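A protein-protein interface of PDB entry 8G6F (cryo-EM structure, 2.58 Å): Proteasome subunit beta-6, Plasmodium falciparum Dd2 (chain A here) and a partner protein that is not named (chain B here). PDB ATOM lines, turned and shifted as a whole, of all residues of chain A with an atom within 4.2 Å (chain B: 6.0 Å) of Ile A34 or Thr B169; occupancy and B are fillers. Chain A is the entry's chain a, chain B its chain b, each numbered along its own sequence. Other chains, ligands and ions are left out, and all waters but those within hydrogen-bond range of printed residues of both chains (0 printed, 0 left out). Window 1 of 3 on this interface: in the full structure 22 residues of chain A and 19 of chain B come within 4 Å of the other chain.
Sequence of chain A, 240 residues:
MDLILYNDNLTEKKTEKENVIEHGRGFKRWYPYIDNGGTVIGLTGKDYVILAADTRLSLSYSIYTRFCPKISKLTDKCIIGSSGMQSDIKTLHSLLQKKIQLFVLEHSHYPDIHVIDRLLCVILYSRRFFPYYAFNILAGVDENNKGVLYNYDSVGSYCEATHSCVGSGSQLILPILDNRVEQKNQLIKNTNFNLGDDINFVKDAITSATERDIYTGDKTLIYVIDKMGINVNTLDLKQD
The side-chain amide oxygen (OE1) of Gln A86 sits at hydrogen-bond distance from the backbone NH (N) of Asn B170 (3.1 Å).
The side-chain hydroxyl (OG) of Ser A87 is in hydrogen-bond range of the backbone carbonyl oxygen (O) of His B167 (2.9 Å).
Tyr A33 touches His B167.
Ile A34 touches His B167.
Ile A34 touches Thr B169.
OD1 of Asn A36 touches OG1 of Thr B169 (3.8 Å).
Phe B171 touches Leu A57 (CD1 to CD2, 3.9 Å).
Gln A86 touches Thr B169.
Gly B168 touches Ser A87.
Ser A87 touches Thr B169.
Of the printed residues of chain A, Asn B170 touches Gln A86 (3.1 Å).
Printed residues of chain B within 4 Å of Asn A36: Thr B169 (3.8 Å).
The nearest residue of chain A that does not touch Thr B169 is Leu A57 (4.1 Å).
The nearest printed residue of chain B that does not touch Leu A57 is Thr B169 (4.1 Å).
The side-chain carboxylate (OD1) of Asp B165 sits at hydrogen-bond distance from the backbone NH (N) of Thr B169, 2.6 Å away.
O of Phe B171 lies within hydrogen-bond range of N of Phe B163 (2.8 Å).
OD1 of Asn A36 sits at hydrogen-bond distance from N of Gln A86 (3.1 Å).
OD1 of Asp B165 is in hydrogen-bond range of N of His B167 (3.1 Å).
The side-chain carboxylate (OD1) of Asp B165 is in hydrogen-bond range of the backbone NH (N) of Gly B168 (3.1 Å).
O of Gly B168 lies close to OD1 of Asn B170.
Along chain B the printed residues that touch a printed residue of chain A span positions 167 to 171.
Of the 10 printed residues of chain A, 6 touch a printed residue of chain B.
Hydrophobic or aromatic side chains of chain A that line the printed part of chain B: Ile A34 and Leu A57.
Among the printed residues, 10 pairs touch across the chains.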
ATOM      1  N   TYR A  33      23.179  -9.916   0.272  1.00  0.00           N
ATOM      2  CA  TYR A  33      23.851 -10.056   1.554  1.00  0.00           C
ATOM      3  C   TYR A  33      22.836 -10.060   2.683  1.00  0.00           C
ATOM      4  O   TYR A  33      21.896  -9.262   2.691  1.00  0.00           O
ATOM      5  CB  TYR A  33      24.842  -8.925   1.799  1.00  0.00           C
ATOM      6  CG  TYR A  33      25.996  -8.888   0.838  1.00  0.00           C
ATOM      7  CD1 TYR A  33      27.050  -9.772   0.960  1.00  0.00           C
ATOM      8  CD2 TYR A  33      26.036  -7.960  -0.182  1.00  0.00           C
ATOM      9  CE1 TYR A  33      28.106  -9.735   0.091  1.00  0.00           C
ATOM     10  CE2 TYR A  33      27.086  -7.917  -1.057  1.00  0.00           C
ATOM     11  CZ  TYR A  33      28.120  -8.804  -0.917  1.00  0.00           C
ATOM     12  OH  TYR A  33      29.177  -8.763  -1.791  1.00  0.00           O
ATOM     13  N   ILE A  34      23.036 -10.967   3.637  1.00  0.00           N
ATOM     14  CA  ILE A  34      22.334 -10.948   4.911  1.00  0.00           C
ATOM     15  C   ILE A  34      23.350 -11.215   6.008  1.00  0.00           C
ATOM     16  O   ILE A  34      24.397 -11.823   5.785  1.00  0.00           O
ATOM     17  CB  ILE A  34      21.191 -11.986   4.991  1.00  0.00           C
ATOM     18  CG1 ILE A  34      21.670 -13.348   4.497  1.00  0.00           C
ATOM     19  CG2 ILE A  34      19.989 -11.518   4.201  1.00  0.00           C
ATOM     20  CD1 ILE A  34      20.774 -14.485   4.904  1.00  0.00           C
ATOM     21  N   ASP A  35      23.027 -10.754   7.205  1.00  0.00           N
ATOM     22  CA  ASP A  35      23.816 -11.045   8.390  1.00  0.00           C
ATOM     23  C   ASP A  35      23.079 -12.091   9.209  1.00  0.00           C
ATOM     24  O   ASP A  35      21.896 -11.925   9.515  1.00  0.00           O
ATOM     25  CB  ASP A  35      24.048  -9.784   9.219  1.00  0.00           C
ATOM     26  CG  ASP A  35      25.330  -9.840  10.016  1.00  0.00           C
ATOM     27  OD1 ASP A  35      25.876 -10.946  10.195  1.00  0.00           O
ATOM     28  OD2 ASP A  35      25.794  -8.775  10.468  1.00  0.00           O
ATOM     29  N   ASN A  36      23.774 -13.173   9.546  1.00  0.00           N
ATOM     30  CA  ASN A  36      23.200 -14.242  10.344  1.00  0.00           C
ATOM     31  C   ASN A  36      23.695 -14.212  11.781  1.00  0.00           C
ATOM     32  O   ASN A  36      23.499 -15.185  12.515  1.00  0.00           O
ATOM     33  CB  ASN A  36      23.500 -15.592   9.700  1.00  0.00           C
ATOM     34  CG  ASN A  36      22.688 -15.824   8.449  1.00  0.00           C
ATOM     35  OD1 ASN A  36      23.207 -15.767   7.339  1.00  0.00           O
ATOM     36  ND2 ASN A  36      21.400 -16.074   8.622  1.00  0.00           N
ATOM     37  N   LEU A  57      22.077 -19.297  14.928  1.00  0.00           N
ATOM     38  CA  LEU A  57      21.875 -18.821  13.566  1.00  0.00           C
ATOM     39  C   LEU A  57      20.546 -18.087  13.503  1.00  0.00           C
ATOM     40  O   LEU A  57      19.517 -18.628  13.916  1.00  0.00           O
ATOM     41  CB  LEU A  57      21.894 -19.980  12.570  1.00  0.00           C
ATOM     42  CG  LEU A  57      21.955 -19.596  11.092  1.00  0.00           C
ATOM     43  CD1 LEU A  57      23.311 -19.040  10.747  1.00  0.00           C
ATOM     44  CD2 LEU A  57      21.634 -20.791  10.221  1.00  0.00           C
ATOM     45  N   LEU A  59      18.013 -14.741  11.550  1.00  0.00           N
ATOM     46  CA  LEU A  59      17.666 -13.961  10.366  1.00  0.00           C
ATOM     47  C   LEU A  59      16.741 -12.835  10.799  1.00  0.00           C
ATOM     48  O   LEU A  59      15.567 -13.076  11.088  1.00  0.00           O
ATOM     49  CB  LEU A  59      16.999 -14.834   9.308  1.00  0.00           C
ATOM     50  CG  LEU A  59      16.586 -14.150   8.004  1.00  0.00           C
ATOM     51  CD1 LEU A  59      17.646 -14.318   6.949  1.00  0.00           C
ATOM     52  CD2 LEU A  59      15.264 -14.710   7.523  1.00  0.00           C
ATOM     53  N   MET A  85      27.540 -13.905   6.834  1.00  0.00           N
ATOM     54  CA  MET A  85      26.543 -14.662   6.089  1.00  0.00           C
ATOM     55  C   MET A  85      26.904 -16.140   6.135  1.00  0.00           C
ATOM     56  O   MET A  85      28.019 -16.525   5.773  1.00  0.00           O
ATOM     57  CB  MET A  85      26.456 -14.171   4.647  1.00  0.00           C
ATOM     58  CG  MET A  85      25.349 -14.832   3.850  1.00  0.00           C
ATOM     59  SD  MET A  85      24.621 -13.776   2.592  1.00  0.00           S
ATOM     60  CE  MET A  85      25.992 -13.626   1.467  1.00  0.00           C
ATOM     61  N   GLN A  86      25.957 -16.966   6.580  1.00  0.00           N
ATOM     62  CA  GLN A  86      26.252 -18.371   6.827  1.00  0.00           C
ATOM     63  C   GLN A  86      26.652 -19.091   5.547  1.00  0.00           C
ATOM     64  O   GLN A  86      27.547 -19.939   5.562  1.00  0.00           O
ATOM     65  CB  GLN A  86      25.042 -19.046   7.468  1.00  0.00           C
ATOM     66  CG  GLN A  86      25.305 -20.449   7.981  1.00  0.00           C
ATOM     67  CD  GLN A  86      24.833 -21.525   7.030  1.00  0.00           C
ATOM     68  OE1 GLN A  86      24.035 -21.275   6.135  1.00  0.00           O
ATOM     69  NE2 GLN A  86      25.325 -22.737   7.224  1.00  0.00           N
ATOM     70  N   SER A  87      25.980 -18.795   4.435  1.00  0.00           N
ATOM     71  CA  SER A  87      26.312 -19.463   3.182  1.00  0.00           C
ATOM     72  C   SER A  87      27.723 -19.114   2.729  1.00  0.00           C
ATOM     73  O   SER A  87      28.479 -19.991   2.292  1.00  0.00           O
ATOM     74  CB  SER A  87      25.294 -19.090   2.111  1.00  0.00           C
ATOM     75  OG  SER A  87      25.289 -17.699   1.880  1.00  0.00           O
ATOM     76  N   TYR A 133      30.952 -12.135   2.651  1.00  0.00           N
ATOM     77  CA  TYR A 133      30.441 -11.464   3.842  1.00  0.00           C
ATOM     78  C   TYR A 133      30.783 -12.339   5.042  1.00  0.00           C
ATOM     79  O   TYR A 133      29.950 -13.057   5.598  1.00  0.00           O
ATOM     80  CB  TYR A 133      28.945 -11.208   3.724  1.00  0.00           C
ATOM     81  CG  TYR A 133      28.382 -10.304   4.801  1.00  0.00           C
ATOM     82  CD1 TYR A 133      29.201  -9.743   5.771  1.00  0.00           C
ATOM     83  CD2 TYR A 133      27.031 -10.010   4.844  1.00  0.00           C
ATOM     84  CE1 TYR A 133      28.691  -8.927   6.747  1.00  0.00           C
ATOM     85  CE2 TYR A 133      26.514  -9.191   5.816  1.00  0.00           C
ATOM     86  CZ  TYR A 133      27.347  -8.651   6.765  1.00  0.00           C
ATOM     87  OH  TYR A 133      26.841  -7.830   7.744  1.00  0.00           O
ATOM     88  N   PHE B 163      16.971 -27.369   5.195  1.00  0.00           N
ATOM     89  CA  PHE B 163      16.398 -26.112   4.752  1.00  0.00           C
ATOM     90  C   PHE B 163      17.428 -25.349   3.937  1.00  0.00           C
ATOM     91  O   PHE B 163      18.607 -25.310   4.306  1.00  0.00           O
ATOM     92  CB  PHE B 163      15.969 -25.280   5.957  1.00  0.00           C
ATOM     93  CG  PHE B 163      15.532 -23.894   5.618  1.00  0.00           C
ATOM     94  CD1 PHE B 163      14.249 -23.645   5.179  1.00  0.00           C
ATOM     95  CD2 PHE B 163      16.405 -22.836   5.745  1.00  0.00           C
ATOM     96  CE1 PHE B 163      13.850 -22.373   4.876  1.00  0.00           C
ATOM     97  CE2 PHE B 163      16.010 -21.567   5.445  1.00  0.00           C
ATOM     98  CZ  PHE B 163      14.730 -21.333   5.008  1.00  0.00           C
ATOM     99  N   VAL B 164      16.976 -24.760   2.826  1.00  0.00           N
ATOM    100  CA  VAL B 164      17.762 -23.834   2.017  1.00  0.00           C
ATOM    101  C   VAL B 164      16.922 -22.589   1.755  1.00  0.00           C
ATOM    102  O   VAL B 164      15.733 -22.694   1.446  1.00  0.00           O
ATOM    103  CB  VAL B 164      18.211 -24.463   0.680  1.00  0.00           C
ATOM    104  CG1 VAL B 164      19.262 -23.598   0.014  1.00  0.00           C
ATOM    105  CG2 VAL B 164      18.739 -25.863   0.894  1.00  0.00           C
ATOM    106  N   ASP B 165      17.534 -21.415   1.875  1.00  0.00           N
ATOM    107  CA  ASP B 165      16.832 -20.155   1.638  1.00  0.00           C
ATOM    108  C   ASP B 165      17.416 -19.432   0.424  1.00  0.00           C
ATOM    109  O   ASP B 165      18.325 -19.923  -0.246  1.00  0.00           O
ATOM    110  CB  ASP B 165      16.865 -19.263   2.885  1.00  0.00           C
ATOM    111  CG  ASP B 165      18.139 -18.454   3.011  1.00  0.00           C
ATOM    112  OD1 ASP B 165      19.156 -18.804   2.387  1.00  0.00           O
ATOM    113  OD2 ASP B 165      18.125 -17.463   3.761  1.00  0.00           O
ATOM    114  N   MET B 166      16.874 -18.242   0.155  1.00  0.00           N
ATOM    115  CA  MET B 166      17.202 -17.518  -1.071  1.00  0.00           C
ATOM    116  C   MET B 166      18.675 -17.145  -1.140  1.00  0.00           C
ATOM    117  O   MET B 166      19.256 -17.121  -2.230  1.00  0.00           O
ATOM    118  CB  MET B 166      16.346 -16.259  -1.176  1.00  0.00           C
ATOM    119  CG  MET B 166      14.918 -16.513  -1.623  1.00  0.00           C
ATOM    120  SD  MET B 166      14.082 -15.058  -2.276  1.00  0.00           S
ATOM    121  CE  MET B 166      15.192 -14.562  -3.583  1.00  0.00           C
ATOM    122  N   HIS B 167      19.291 -16.839  -0.005  1.00  0.00           N
ATOM    123  CA  HIS B 167      20.695 -16.463   0.043  1.00  0.00           C
ATOM    124  C   HIS B 167      21.621 -17.663   0.142  1.00  0.00           C
ATOM    125  O   HIS B 167      22.825 -17.484   0.336  1.00  0.00           O
ATOM    126  CB  HIS B 167      20.947 -15.526   1.221  1.00  0.00           C
ATOM    127  CG  HIS B 167      20.480 -14.127   0.988  1.00  0.00           C
ATOM    128  ND1 HIS B 167      19.210 -13.705   1.313  1.00  0.00           N
ATOM    129  CD2 HIS B 167      21.108 -13.056   0.453  1.00  0.00           C
ATOM    130  CE1 HIS B 167      19.079 -12.431   0.994  1.00  0.00           C
ATOM    131  NE2 HIS B 167      20.216 -12.014   0.471  1.00  0.00           N
ATOM    132  N   GLY B 168      21.094 -18.874   0.020  1.00  0.00           N
ATOM    133  CA  GLY B 168      21.898 -20.062   0.149  1.00  0.00           C
ATOM    134  C   GLY B 168      22.126 -20.516   1.567  1.00  0.00           C
ATOM    135  O   GLY B 168      22.831 -21.510   1.772  1.00  0.00           O
ATOM    136  N   THR B 169      21.574 -19.816   2.555  1.00  0.00           N
ATOM    137  CA  THR B 169      21.667 -20.274   3.932  1.00  0.00           C
ATOM    138  C   THR B 169      20.991 -21.629   4.055  1.00  0.00           C
ATOM    139  O   THR B 169      19.850 -21.808   3.620  1.00  0.00           O
ATOM    140  CB  THR B 169      21.017 -19.262   4.874  1.00  0.00           C
ATOM    141  OG1 THR B 169      21.646 -17.987   4.708  1.00  0.00           O
ATOM    142  CG2 THR B 169      21.153 -19.698   6.318  1.00  0.00           C
ATOM    143  N   ASN B 170      21.699 -22.587   4.642  1.00  0.00           N
ATOM    144  CA  ASN B 170      21.237 -23.962   4.665  1.00  0.00           C
ATOM    145  C   ASN B 170      21.607 -24.612   5.985  1.00  0.00           C
ATOM    146  O   ASN B 170      22.656 -24.331   6.565  1.00  0.00           O
ATOM    147  CB  ASN B 170      21.830 -24.781   3.509  1.00  0.00           C
ATOM    148  CG  ASN B 170      23.340 -24.818   3.533  1.00  0.00           C
ATOM    149  OD1 ASN B 170      24.001 -23.791   3.416  1.00  0.00           O
ATOM    150  ND2 ASN B 170      23.895 -26.005   3.688  1.00  0.00           N
ATOM    151  N   PHE B 171      20.731 -25.493   6.449  1.00  0.00           N
ATOM    152  CA  PHE B 171      20.996 -26.239   7.675  1.00  0.00           C
ATOM    153  C   PHE B 171      20.031 -27.411   7.748  1.00  0.00           C
ATOM    154  O   PHE B 171      19.286 -27.678   6.809  1.00  0.00           O
ATOM    155  CB  PHE B 171      20.894 -25.337   8.911  1.00  0.00           C
ATOM    156  CG  PHE B 171      19.599 -24.598   9.017  1.00  0.00           C
ATOM    157  CD1 PHE B 171      19.424 -23.393   8.369  1.00  0.00           C
ATOM    158  CD2 PHE B 171      18.558 -25.101   9.770  1.00  0.00           C
ATOM    159  CE1 PHE B 171      18.241 -22.713   8.464  1.00  0.00           C
ATOM    160  CE2 PHE B 171      17.372 -24.422   9.866  1.00  0.00           C
ATOM    161  CZ  PHE B 171      17.213 -23.229   9.211  1.00  0.00           C
